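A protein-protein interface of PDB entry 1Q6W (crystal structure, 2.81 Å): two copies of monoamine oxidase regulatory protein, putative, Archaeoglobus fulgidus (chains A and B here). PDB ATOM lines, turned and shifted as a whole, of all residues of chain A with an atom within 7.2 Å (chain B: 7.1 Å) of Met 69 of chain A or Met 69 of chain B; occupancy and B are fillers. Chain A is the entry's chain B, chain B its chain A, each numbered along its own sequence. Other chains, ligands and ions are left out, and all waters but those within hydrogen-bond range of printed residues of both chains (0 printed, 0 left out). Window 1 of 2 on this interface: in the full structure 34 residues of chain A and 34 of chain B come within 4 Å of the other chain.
The backbone carbonyl oxygen (O) of Ile 98 of chain B is in hydrogen-bond range of the backbone NH (N) of Val 101 of chain A (3.0 Å).
N of Val 101 of chain B is in hydrogen-bond range of O of Ile 98 of chain A, 2.9 Å away.
O of Met 69 of chain B is in hydrogen-bond range of OG of Ser 73 of chain B.
O of Phe 39 of chain B sits at hydrogen-bond distance from OG1 of Thr 43 of chain B, at 3.0 Å.
The backbone carbonyl oxygen of Phe 39 of chain A lies within hydrogen-bond range of the side-chain hydroxyl of Thr 43 of chain A.
The side-chain hydroxyl (OG) of Ser 73 of chain A lies within hydrogen-bond range of the backbone carbonyl oxygen (O) of Met 69 of chain A.
Among the printed residues, merely in contact across the chains: Phe 39 of chain A with Ser 73 of chain B (3.3 Å), Thr 43 of chain A with Ser 73 of chain B (3.7 Å), Met 69 of chain A with Met 69 of chain B (3.3 Å), Met 69 of chain A with Leu 72 of chain B (3.6 Å), Met 69 of chain A with Ser 73 of chain B (3.4 Å), Met 69 of chain A with Leu 76 of chain B (3.8 Å), Met 69 of chain A with Ile 98 of chain B (3.6 Å), Leu 72 of chain A with Met 69 of chain B (3.5 Å), Ser 73 of chain A with Phe 39 of chain B (3.4 Å), Ser 73 of chain A with Thr 43 of chain B (3.6 Å), Ser 73 of chain A with Met 69 of chain B (3.5 Å), Leu 76 of chain A with Met 69 of chain B (3.7 Å), Phe 95 of chain A with Phe 103 of chain B (3.4 Å), Ile 98 of chain A with Met 69 of chain B (3.5 Å) and Phe 103 of chain A with Phe 95 of chain B (3.4 Å).
Printed residues of chain B within 4 Å of Met 69 of chain A: Met 69 (3.3 Å), Leu 72 (3.6 Å), Ser 73 (3.4 Å), Leu 76 (3.8 Å) and Ile 98 (3.6 Å).
No residue of chain B comes within 4 Å of Gly 68 of chain A.
Of the printed residues of chain B, Ile 98 of chain A touches Met 69 and Val 101.
Of the printed residues of chain B, Phe 103 of chain A touches Phe 95.
His 50 of chain A touches none of the printed residues of chain B.
Ile 74 of chain A touches none of the printed residues of chain B.
The nearest residue of chain B that does not touch Met 69 of chain A is Phe 95 of chain B (4.3 Å).
The nearest residue of chain A that does not touch Met 69 of chain B is Phe 95 of chain A (4.2 Å).
Of the 18 printed residues of chain B, 10 touch a printed residue of chain A.
Hydrophobic or aromatic side chains of chain B that line the printed part of chain A: Phe 39, Met 69, Leu 72, Leu 76, Phe 95, Ile 98, Val 101 and Phe 103.
Along chain B the printed residues that touch a printed residue of chain A span positions 39 to 103.
Hydrophobic or aromatic side chains of chain A within 4 Å of the printed part of chain B: Phe 39, Met 69, Leu 72, Leu 76, Phe 95, Ile 98, Val 101 and Phe 103.
Among the printed residues, 17 pairs touch across the chains.
Phe 39 of chain A touches Ser 73 of chain B, and with the chains exchanged Ser 73 of chain A touches Phe 39 of chain B.
Met 69 of chain A touches Leu 76 of chain B, and with the chains exchanged Leu 76 of chain A touches Met 69 of chain B.
Phe 95 of chain A touches Phe 103 of chain B, and with the chains exchanged Phe 103 of chain A touches Phe 95 of chain B.
Ile 98 of chain A touches Val 101 of chain B, and with the chains exchanged Val 101 of chain A touches Ile 98 of chain B.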
ATOM      1  N   PHE A  39       4.902 -15.474 -15.015  1.00  0.00           N
ATOM      2  CA  PHE A  39       5.046 -15.798 -13.608  1.00  0.00           C
ATOM      3  C   PHE A  39       5.758 -17.124 -13.471  1.00  0.00           C
ATOM      4  O   PHE A  39       6.611 -17.294 -12.599  1.00  0.00           O
ATOM      5  CB  PHE A  39       3.682 -15.860 -12.917  1.00  0.00           C
ATOM      6  CG  PHE A  39       3.771 -15.882 -11.427  1.00  0.00           C
ATOM      7  CD1 PHE A  39       4.052 -14.708 -10.712  1.00  0.00           C
ATOM      8  CD2 PHE A  39       3.632 -17.077 -10.729  1.00  0.00           C
ATOM      9  CE1 PHE A  39       4.197 -14.723  -9.314  1.00  0.00           C
ATOM     10  CE2 PHE A  39       3.776 -17.107  -9.317  1.00  0.00           C
ATOM     11  CZ  PHE A  39       4.059 -15.926  -8.612  1.00  0.00           C
ATOM     12  N   THR A  43       9.456 -17.538 -11.570  1.00  0.00           N
ATOM     13  CA  THR A  43       9.584 -18.397 -10.398  1.00  0.00           C
ATOM     14  C   THR A  43      10.122 -19.783 -10.736  1.00  0.00           C
ATOM     15  O   THR A  43      10.217 -20.643  -9.854  1.00  0.00           O
ATOM     16  CB  THR A  43       8.223 -18.566  -9.708  1.00  0.00           C
ATOM     17  OG1 THR A  43       7.347 -19.285 -10.585  1.00  0.00           O
ATOM     18  CG2 THR A  43       7.592 -17.199  -9.388  1.00  0.00           C
ATOM     19  N   HIS A  50      -1.096 -25.173 -14.129  1.00  0.00           N
ATOM     20  CA  HIS A  50      -1.010 -23.872 -14.776  1.00  0.00           C
ATOM     21  C   HIS A  50      -0.405 -23.940 -16.158  1.00  0.00           C
ATOM     22  O   HIS A  50      -0.815 -23.192 -17.043  1.00  0.00           O
ATOM     23  CB  HIS A  50      -0.165 -22.917 -13.940  1.00  0.00           C
ATOM     24  CG  HIS A  50      -0.532 -22.896 -12.493  1.00  0.00           C
ATOM     25  ND1 HIS A  50      -1.781 -22.519 -12.053  1.00  0.00           N
ATOM     26  CD2 HIS A  50       0.182 -23.208 -11.387  1.00  0.00           C
ATOM     27  CE1 HIS A  50      -1.820 -22.600 -10.736  1.00  0.00           C
ATOM     28  NE2 HIS A  50      -0.641 -23.017 -10.308  1.00  0.00           N
ATOM     29  N   ALA A  66      -4.831 -19.596 -13.319  1.00  0.00           N
ATOM     30  CA  ALA A  66      -3.729 -18.740 -12.909  1.00  0.00           C
ATOM     31  C   ALA A  66      -3.187 -19.170 -11.553  1.00  0.00           C
ATOM     32  O   ALA A  66      -3.875 -19.814 -10.772  1.00  0.00           O
ATOM     33  CB  ALA A  66      -4.192 -17.300 -12.862  1.00  0.00           C
ATOM     34  N   GLN A  67      -1.935 -18.836 -11.288  1.00  0.00           N
ATOM     35  CA  GLN A  67      -1.326 -19.171 -10.012  1.00  0.00           C
ATOM     36  C   GLN A  67      -1.883 -18.202  -8.975  1.00  0.00           C
ATOM     37  O   GLN A  67      -2.095 -17.019  -9.261  1.00  0.00           O
ATOM     38  CB  GLN A  67       0.202 -19.031 -10.087  1.00  0.00           C
ATOM     39  CG  GLN A  67       0.842 -19.848 -11.193  1.00  0.00           C
ATOM     40  CD  GLN A  67       0.988 -19.090 -12.507  1.00  0.00           C
ATOM     41  OE1 GLN A  67       0.122 -18.303 -12.892  1.00  0.00           O
ATOM     42  NE2 GLN A  67       2.084 -19.341 -13.208  1.00  0.00           N
ATOM     43  N   GLY A  68      -2.124 -18.709  -7.772  1.00  0.00           N
ATOM     44  CA  GLY A  68      -2.653 -17.864  -6.723  1.00  0.00           C
ATOM     45  C   GLY A  68      -1.687 -16.734  -6.431  1.00  0.00           C
ATOM     46  O   GLY A  68      -2.103 -15.589  -6.260  1.00  0.00           O
ATOM     47  N   MET A  69      -0.395 -17.044  -6.364  1.00  0.00           N
ATOM     48  CA  MET A  69       0.590 -16.005  -6.111  1.00  0.00           C
ATOM     49  C   MET A  69       0.567 -14.924  -7.206  1.00  0.00           C
ATOM     50  O   MET A  69       0.887 -13.759  -6.955  1.00  0.00           O
ATOM     51  CB  MET A  69       1.986 -16.619  -6.015  1.00  0.00           C
ATOM     52  CG  MET A  69       2.263 -17.284  -4.685  1.00  0.00           C
ATOM     53  SD  MET A  69       1.958 -16.071  -3.199  1.00  0.00           S
ATOM     54  CE  MET A  69       3.532 -14.955  -3.400  1.00  0.00           C
ATOM     55  N   LEU A  70       0.198 -15.314  -8.428  1.00  0.00           N
ATOM     56  CA  LEU A  70       0.134 -14.361  -9.526  1.00  0.00           C
ATOM     57  C   LEU A  70      -1.015 -13.393  -9.285  1.00  0.00           C
ATOM     58  O   LEU A  70      -0.845 -12.180  -9.381  1.00  0.00           O
ATOM     59  CB  LEU A  70      -0.071 -15.080 -10.865  1.00  0.00           C
ATOM     60  CG  LEU A  70      -0.335 -14.138 -12.057  1.00  0.00           C
ATOM     61  CD1 LEU A  70       0.846 -13.229 -12.269  1.00  0.00           C
ATOM     62  CD2 LEU A  70      -0.619 -14.923 -13.307  1.00  0.00           C
ATOM     63  N   VAL A  71      -2.188 -13.947  -8.973  1.00  0.00           N
ATOM     64  CA  VAL A  71      -3.363 -13.130  -8.711  1.00  0.00           C
ATOM     65  C   VAL A  71      -3.107 -12.174  -7.550  1.00  0.00           C
ATOM     66  O   VAL A  71      -3.465 -10.997  -7.627  1.00  0.00           O
ATOM     67  CB  VAL A  71      -4.594 -13.982  -8.396  1.00  0.00           C
ATOM     68  CG1 VAL A  71      -5.808 -13.083  -8.268  1.00  0.00           C
ATOM     69  CG2 VAL A  71      -4.823 -14.999  -9.514  1.00  0.00           C
ATOM     70  N   LEU A  72      -2.462 -12.673  -6.495  1.00  0.00           N
ATOM     71  CA  LEU A  72      -2.141 -11.849  -5.354  1.00  0.00           C
ATOM     72  C   LEU A  72      -1.199 -10.715  -5.763  1.00  0.00           C
ATOM     73  O   LEU A  72      -1.429  -9.540  -5.436  1.00  0.00           O
ATOM     74  CB  LEU A  72      -1.496 -12.687  -4.269  1.00  0.00           C
ATOM     75  CG  LEU A  72      -1.173 -11.999  -2.933  1.00  0.00           C
ATOM     76  CD1 LEU A  72      -2.423 -11.223  -2.440  1.00  0.00           C
ATOM     77  CD2 LEU A  72      -0.703 -13.046  -1.921  1.00  0.00           C
ATOM     78  N   SER A  73      -0.155 -11.052  -6.500  1.00  0.00           N
ATOM     79  CA  SER A  73       0.818 -10.051  -6.937  1.00  0.00           C
ATOM     80  C   SER A  73       0.202  -8.982  -7.815  1.00  0.00           C
ATOM     81  O   SER A  73       0.461  -7.792  -7.607  1.00  0.00           O
ATOM     82  CB  SER A  73       1.974 -10.701  -7.696  1.00  0.00           C
ATOM     83  OG  SER A  73       2.728 -11.537  -6.849  1.00  0.00           O
ATOM     84  N   ILE A  74      -0.603  -9.396  -8.794  1.00  0.00           N
ATOM     85  CA  ILE A  74      -1.230  -8.430  -9.685  1.00  0.00           C
ATOM     86  C   ILE A  74      -2.189  -7.545  -8.881  1.00  0.00           C
ATOM     87  O   ILE A  74      -2.277  -6.343  -9.115  1.00  0.00           O
ATOM     88  CB  ILE A  74      -1.988  -9.135 -10.847  1.00  0.00           C
ATOM     89  CG1 ILE A  74      -0.975  -9.787 -11.802  1.00  0.00           C
ATOM     90  CG2 ILE A  74      -2.857  -8.127 -11.615  1.00  0.00           C
ATOM     91  CD1 ILE A  74      -1.616 -10.422 -13.039  1.00  0.00           C
ATOM     92  N   ALA A  75      -2.882  -8.148  -7.913  1.00  0.00           N
ATOM     93  CA  ALA A  75      -3.821  -7.414  -7.073  1.00  0.00           C
ATOM     94  C   ALA A  75      -3.111  -6.316  -6.281  1.00  0.00           C
ATOM     95  O   ALA A  75      -3.453  -5.135  -6.390  1.00  0.00           O
ATOM     96  CB  ALA A  75      -4.512  -8.370  -6.119  1.00  0.00           C
ATOM     97  N   LEU A  76      -2.128  -6.704  -5.475  1.00  0.00           N
ATOM     98  CA  LEU A  76      -1.398  -5.721  -4.686  1.00  0.00           C
ATOM     99  C   LEU A  76      -0.821  -4.652  -5.597  1.00  0.00           C
ATOM    100  O   LEU A  76      -0.777  -3.475  -5.254  1.00  0.00           O
ATOM    101  CB  LEU A  76      -0.282  -6.403  -3.918  1.00  0.00           C
ATOM    102  CG  LEU A  76      -0.772  -7.359  -2.840  1.00  0.00           C
ATOM    103  CD1 LEU A  76       0.409  -8.167  -2.290  1.00  0.00           C
ATOM    104  CD2 LEU A  76      -1.500  -6.543  -1.742  1.00  0.00           C
ATOM    105  N   PHE A  95       7.047  -3.009   3.929  1.00  0.00           N
ATOM    106  CA  PHE A  95       5.950  -3.941   3.770  1.00  0.00           C
ATOM    107  C   PHE A  95       6.115  -4.802   5.013  1.00  0.00           C
ATOM    108  O   PHE A  95       7.059  -5.570   5.117  1.00  0.00           O
ATOM    109  CB  PHE A  95       6.140  -4.761   2.487  1.00  0.00           C
ATOM    110  CG  PHE A  95       4.923  -5.547   2.073  1.00  0.00           C
ATOM    111  CD1 PHE A  95       4.874  -6.153   0.821  1.00  0.00           C
ATOM    112  CD2 PHE A  95       3.813  -5.659   2.921  1.00  0.00           C
ATOM    113  CE1 PHE A  95       3.746  -6.853   0.408  1.00  0.00           C
ATOM    114  CE2 PHE A  95       2.683  -6.355   2.522  1.00  0.00           C
ATOM    115  CZ  PHE A  95       2.646  -6.954   1.259  1.00  0.00           C
ATOM    116  N   ILE A  98       1.920 -10.134   5.535  1.00  0.00           N
ATOM    117  CA  ILE A  98       0.646 -10.511   4.968  1.00  0.00           C
ATOM    118  C   ILE A  98       0.221 -11.503   6.002  1.00  0.00           C
ATOM    119  O   ILE A  98       0.963 -12.448   6.287  1.00  0.00           O
ATOM    120  CB  ILE A  98       0.794 -11.223   3.637  1.00  0.00           C
ATOM    121  CG1 ILE A  98       1.598 -10.350   2.675  1.00  0.00           C
ATOM    122  CG2 ILE A  98      -0.578 -11.535   3.076  1.00  0.00           C
ATOM    123  CD1 ILE A  98       1.933 -11.055   1.401  1.00  0.00           C
ATOM    124  N   VAL A 101      -4.238 -14.979   3.580  1.00  0.00           N
ATOM    125  CA  VAL A 101      -4.542 -14.994   2.177  1.00  0.00           C
ATOM    126  C   VAL A 101      -5.388 -16.218   1.960  1.00  0.00           C
ATOM    127  O   VAL A 101      -5.003 -17.323   2.352  1.00  0.00           O
ATOM    128  CB  VAL A 101      -3.281 -15.079   1.290  1.00  0.00           C
ATOM    129  CG1 VAL A 101      -3.689 -14.975  -0.175  1.00  0.00           C
ATOM    130  CG2 VAL A 101      -2.324 -13.943   1.618  1.00  0.00           C
ATOM    131  N   PHE A 103      -7.492 -18.264  -1.047  1.00  0.00           N
ATOM    132  CA  PHE A 103      -7.757 -18.442  -2.464  1.00  0.00           C
ATOM    133  C   PHE A 103      -9.137 -19.069  -2.549  1.00  0.00           C
ATOM    134  O   PHE A 103      -9.305 -20.271  -2.370  1.00  0.00           O
ATOM    135  CB  PHE A 103      -6.679 -19.339  -3.084  1.00  0.00           C
ATOM    136  CG  PHE A 103      -5.292 -18.781  -2.946  1.00  0.00           C
ATOM    137  CD1 PHE A 103      -4.366 -19.378  -2.086  1.00  0.00           C
ATOM    138  CD2 PHE A 103      -4.924 -17.630  -3.630  1.00  0.00           C
ATOM    139  CE1 PHE A 103      -3.088 -18.837  -1.906  1.00  0.00           C
ATOM    140  CE2 PHE A 103      -3.656 -17.075  -3.466  1.00  0.00           C
ATOM    141  CZ  PHE A 103      -2.735 -17.677  -2.603  1.00  0.00           C
ATOM    142  N   LEU A 147     -10.204 -13.911  -4.441  1.00  0.00           N
ATOM    143  CA  LEU A 147      -9.165 -13.924  -3.437  1.00  0.00           C
ATOM    144  C   LEU A 147      -9.387 -12.850  -2.381  1.00  0.00           C
ATOM    145  O   LEU A 147      -9.950 -11.780  -2.644  1.00  0.00           O
ATOM    146  CB  LEU A 147      -7.807 -13.741  -4.121  1.00  0.00           C
ATOM    147  CG  LEU A 147      -6.526 -13.685  -3.291  1.00  0.00           C
ATOM    148  CD1 LEU A 147      -5.370 -14.105  -4.167  1.00  0.00           C
ATOM    149  CD2 LEU A 147      -6.302 -12.280  -2.726  1.00  0.00           C
ATOM    150  N   PHE B  39       9.392  -8.498 -12.075  1.00  0.00           N
ATOM    151  CA  PHE B  39       8.272  -8.505 -11.152  1.00  0.00           C
ATOM    152  C   PHE B  39       7.527  -7.179 -11.247  1.00  0.00           C
ATOM    153  O   PHE B  39       6.298  -7.151 -11.248  1.00  0.00           O
ATOM    154  CB  PHE B  39       8.744  -8.741  -9.729  1.00  0.00           C
ATOM    155  CG  PHE B  39       7.636  -9.069  -8.787  1.00  0.00           C
ATOM    156  CD1 PHE B  39       7.063 -10.334  -8.790  1.00  0.00           C
ATOM    157  CD2 PHE B  39       7.130  -8.102  -7.917  1.00  0.00           C
ATOM    158  CE1 PHE B  39       6.002 -10.626  -7.943  1.00  0.00           C
ATOM    159  CE2 PHE B  39       6.072  -8.392  -7.069  1.00  0.00           C
ATOM    160  CZ  PHE B  39       5.510  -9.648  -7.084  1.00  0.00           C
ATOM    161  N   THR B  43       3.540  -6.848 -12.423  1.00  0.00           N
ATOM    162  CA  THR B  43       2.557  -6.290 -11.511  1.00  0.00           C
ATOM    163  C   THR B  43       2.264  -4.812 -11.784  1.00  0.00           C
ATOM    164  O   THR B  43       1.452  -4.187 -11.069  1.00  0.00           O
ATOM    165  CB  THR B  43       3.025  -6.439 -10.042  1.00  0.00           C
ATOM    166  OG1 THR B  43       4.164  -5.598  -9.805  1.00  0.00           O
ATOM    167  CG2 THR B  43       3.390  -7.880  -9.740  1.00  0.00           C
ATOM    168  N   ALA B  66      14.727  -5.944  -3.174  1.00  0.00           N
ATOM    169  CA  ALA B  66      13.738  -6.759  -3.858  1.00  0.00           C
ATOM    170  C   ALA B  66      12.368  -6.624  -3.225  1.00  0.00           C
ATOM    171  O   ALA B  66      12.259  -6.299  -2.057  1.00  0.00           O
ATOM    172  CB  ALA B  66      14.170  -8.217  -3.845  1.00  0.00           C
ATOM    173  N   GLN B  67      11.321  -6.874  -4.001  1.00  0.00           N
ATOM    174  CA  GLN B  67       9.978  -6.792  -3.478  1.00  0.00           C
ATOM    175  C   GLN B  67       9.742  -8.014  -2.608  1.00  0.00           C
ATOM    176  O   GLN B  67      10.190  -9.106  -2.943  1.00  0.00           O
ATOM    177  CB  GLN B  67       8.952  -6.761  -4.609  1.00  0.00           C
ATOM    178  CG  GLN B  67       9.158  -5.635  -5.596  1.00  0.00           C
ATOM    179  CD  GLN B  67      10.051  -6.035  -6.780  1.00  0.00           C
ATOM    180  OE1 GLN B  67      11.042  -6.765  -6.607  1.00  0.00           O
ATOM    181  NE2 GLN B  67       9.713  -5.540  -7.982  1.00  0.00           N
ATOM    182  N   GLY B  68       9.041  -7.840  -1.489  1.00  0.00           N
ATOM    183  CA  GLY B  68       8.755  -8.972  -0.626  1.00  0.00           C
ATOM    184  C   GLY B  68       7.953 -10.031  -1.352  1.00  0.00           C
ATOM    185  O   GLY B  68       8.218 -11.218  -1.175  1.00  0.00           O
ATOM    186  N   MET B  69       6.965  -9.614  -2.153  1.00  0.00           N
ATOM    187  CA  MET B  69       6.172 -10.572  -2.924  1.00  0.00           C
ATOM    188  C   MET B  69       7.054 -11.350  -3.902  1.00  0.00           C
ATOM    189  O   MET B  69       6.763 -12.510  -4.205  1.00  0.00           O
ATOM    190  CB  MET B  69       5.065  -9.862  -3.699  1.00  0.00           C
ATOM    191  CG  MET B  69       3.864  -9.493  -2.846  1.00  0.00           C
ATOM    192  SD  MET B  69       3.113 -11.012  -1.946  1.00  0.00           S
ATOM    193  CE  MET B  69       2.259 -11.881  -3.446  1.00  0.00           C
ATOM    194  N   LEU B  70       8.129 -10.712  -4.391  1.00  0.00           N
ATOM    195  CA  LEU B  70       9.037 -11.370  -5.308  1.00  0.00           C
ATOM    196  C   LEU B  70       9.793 -12.481  -4.579  1.00  0.00           C
ATOM    197  O   LEU B  70       9.884 -13.620  -5.057  1.00  0.00           O
ATOM    198  CB  LEU B  70      10.029 -10.373  -5.904  1.00  0.00           C
ATOM    199  CG  LEU B  70      11.165 -11.017  -6.715  1.00  0.00           C
ATOM    200  CD1 LEU B  70      10.597 -11.769  -7.922  1.00  0.00           C
ATOM    201  CD2 LEU B  70      12.149  -9.954  -7.129  1.00  0.00           C
ATOM    202  N   VAL B  71      10.336 -12.146  -3.417  1.00  0.00           N
ATOM    203  CA  VAL B  71      11.076 -13.133  -2.648  1.00  0.00           C
ATOM    204  C   VAL B  71      10.183 -14.316  -2.272  1.00  0.00           C
ATOM    205  O   VAL B  71      10.610 -15.479  -2.307  1.00  0.00           O
ATOM    206  CB  VAL B  71      11.669 -12.518  -1.362  1.00  0.00           C
ATOM    207  CG1 VAL B  71      12.516 -13.555  -0.655  1.00  0.00           C
ATOM    208  CG2 VAL B  71      12.524 -11.293  -1.709  1.00  0.00           C
ATOM    209  N   LEU B  72       8.939 -14.019  -1.918  1.00  0.00           N
ATOM    210  CA  LEU B  72       8.009 -15.063  -1.540  1.00  0.00           C
ATOM    211  C   LEU B  72       7.727 -15.966  -2.741  1.00  0.00           C
ATOM    212  O   LEU B  72       7.771 -17.183  -2.637  1.00  0.00           O
ATOM    213  CB  LEU B  72       6.714 -14.437  -1.009  1.00  0.00           C
ATOM    214  CG  LEU B  72       5.636 -15.408  -0.498  1.00  0.00           C
ATOM    215  CD1 LEU B  72       6.237 -16.378   0.525  1.00  0.00           C
ATOM    216  CD2 LEU B  72       4.469 -14.622   0.103  1.00  0.00           C
ATOM    217  N   SER B  73       7.456 -15.358  -3.887  1.00  0.00           N
ATOM    218  CA  SER B  73       7.181 -16.098  -5.112  1.00  0.00           C
ATOM    219  C   SER B  73       8.363 -16.975  -5.533  1.00  0.00           C
ATOM    220  O   SER B  73       8.188 -18.155  -5.852  1.00  0.00           O
ATOM    221  CB  SER B  73       6.842 -15.138  -6.248  1.00  0.00           C
ATOM    222  OG  SER B  73       5.597 -14.512  -6.018  1.00  0.00           O
ATOM    223  N   ILE B  74       9.565 -16.403  -5.549  1.00  0.00           N
ATOM    224  CA  ILE B  74      10.719 -17.191  -5.914  1.00  0.00           C
ATOM    225  C   ILE B  74      10.915 -18.338  -4.932  1.00  0.00           C
ATOM    226  O   ILE B  74      11.230 -19.450  -5.323  1.00  0.00           O
ATOM    227  CB  ILE B  74      11.992 -16.335  -5.993  1.00  0.00           C
ATOM    228  CG1 ILE B  74      11.891 -15.358  -7.194  1.00  0.00           C
ATOM    229  CG2 ILE B  74      13.211 -17.250  -6.150  1.00  0.00           C
ATOM    230  CD1 ILE B  74      13.144 -14.520  -7.439  1.00  0.00           C
ATOM    231  N   ALA B  75      10.691 -18.071  -3.647  1.00  0.00           N
ATOM    232  CA  ALA B  75      10.836 -19.092  -2.604  1.00  0.00           C
ATOM    233  C   ALA B  75       9.886 -20.261  -2.837  1.00  0.00           C
ATOM    234  O   ALA B  75      10.327 -21.398  -2.983  1.00  0.00           O
ATOM    235  CB  ALA B  75      10.580 -18.481  -1.246  1.00  0.00           C
ATOM    236  N   LEU B  76       8.581 -19.983  -2.859  1.00  0.00           N
ATOM    237  CA  LEU B  76       7.608 -21.038  -3.089  1.00  0.00           C
ATOM    238  C   LEU B  76       7.956 -21.788  -4.375  1.00  0.00           C
ATOM    239  O   LEU B  76       7.817 -23.004  -4.467  1.00  0.00           O
ATOM    240  CB  LEU B  76       6.224 -20.440  -3.198  1.00  0.00           C
ATOM    241  CG  LEU B  76       5.697 -19.855  -1.881  1.00  0.00           C
ATOM    242  CD1 LEU B  76       4.383 -19.099  -2.106  1.00  0.00           C
ATOM    243  CD2 LEU B  76       5.515 -20.993  -0.846  1.00  0.00           C
ATOM    244  N   PHE B  95      -4.080 -24.887  -3.814  1.00  0.00           N
ATOM    245  CA  PHE B  95      -3.298 -24.054  -2.927  1.00  0.00           C
ATOM    246  C   PHE B  95      -4.371 -23.498  -1.998  1.00  0.00           C
ATOM    247  O   PHE B  95      -5.168 -22.658  -2.398  1.00  0.00           O
ATOM    248  CB  PHE B  95      -2.638 -22.933  -3.723  1.00  0.00           C
ATOM    249  CG  PHE B  95      -1.560 -22.208  -2.974  1.00  0.00           C
ATOM    250  CD1 PHE B  95      -0.723 -21.310  -3.632  1.00  0.00           C
ATOM    251  CD2 PHE B  95      -1.363 -22.424  -1.608  1.00  0.00           C
ATOM    252  CE1 PHE B  95       0.302 -20.635  -2.943  1.00  0.00           C
ATOM    253  CE2 PHE B  95      -0.353 -21.760  -0.919  1.00  0.00           C
ATOM    254  CZ  PHE B  95       0.485 -20.865  -1.584  1.00  0.00           C
ATOM    255  N   ILE B  98      -2.294 -18.918   2.625  1.00  0.00           N
ATOM    256  CA  ILE B  98      -1.022 -18.535   3.206  1.00  0.00           C
ATOM    257  C   ILE B  98      -1.427 -17.818   4.472  1.00  0.00           C
ATOM    258  O   ILE B  98      -1.911 -16.693   4.421  1.00  0.00           O
ATOM    259  CB  ILE B  98      -0.268 -17.578   2.305  1.00  0.00           C
ATOM    260  CG1 ILE B  98      -0.114 -18.192   0.917  1.00  0.00           C
ATOM    261  CG2 ILE B  98       1.079 -17.284   2.895  1.00  0.00           C
ATOM    262  CD1 ILE B  98       0.659 -17.321  -0.029  1.00  0.00           C
ATOM    263  N   VAL B 101       3.023 -14.446   6.809  1.00  0.00           N
ATOM    264  CA  VAL B 101       4.216 -14.122   6.079  1.00  0.00           C
ATOM    265  C   VAL B 101       4.857 -12.975   6.807  1.00  0.00           C
ATOM    266  O   VAL B 101       4.216 -11.941   7.035  1.00  0.00           O
ATOM    267  CB  VAL B 101       3.904 -13.685   4.614  1.00  0.00           C
ATOM    268  CG1 VAL B 101       5.201 -13.383   3.861  1.00  0.00           C
ATOM    269  CG2 VAL B 101       3.139 -14.774   3.892  1.00  0.00           C
ATOM    270  N   PHE B 103       8.206 -10.450   6.720  1.00  0.00           N
ATOM    271  CA  PHE B 103       9.372  -9.963   5.997  1.00  0.00           C
ATOM    272  C   PHE B 103      10.376  -9.507   7.051  1.00  0.00           C
ATOM    273  O   PHE B 103      10.267  -8.439   7.611  1.00  0.00           O
ATOM    274  CB  PHE B 103       8.946  -8.831   5.067  1.00  0.00           C
ATOM    275  CG  PHE B 103       7.918  -9.256   4.047  1.00  0.00           C
ATOM    276  CD1 PHE B 103       6.607  -8.771   4.111  1.00  0.00           C
ATOM    277  CD2 PHE B 103       8.242 -10.183   3.053  1.00  0.00           C
ATOM    278  CE1 PHE B 103       5.637  -9.197   3.208  1.00  0.00           C
ATOM    279  CE2 PHE B 103       7.280 -10.620   2.142  1.00  0.00           C
ATOM    280  CZ  PHE B 103       5.978 -10.131   2.212  1.00  0.00           C
ATOM    281  N   LEU B 147      12.947 -14.117   5.275  1.00  0.00           N
ATOM    282  CA  LEU B 147      11.501 -14.217   5.189  1.00  0.00           C
ATOM    283  C   LEU B 147      11.008 -15.519   5.786  1.00  0.00           C
ATOM    284  O   LEU B 147      11.682 -16.541   5.718  1.00  0.00           O
ATOM    285  CB  LEU B 147      11.054 -14.104   3.722  1.00  0.00           C
ATOM    286  CG  LEU B 147       9.566 -14.218   3.361  1.00  0.00           C
ATOM    287  CD1 LEU B 147       9.327 -13.510   2.046  1.00  0.00           C
ATOM    288  CD2 LEU B 147       9.123 -15.675   3.274  1.00  0.00           C
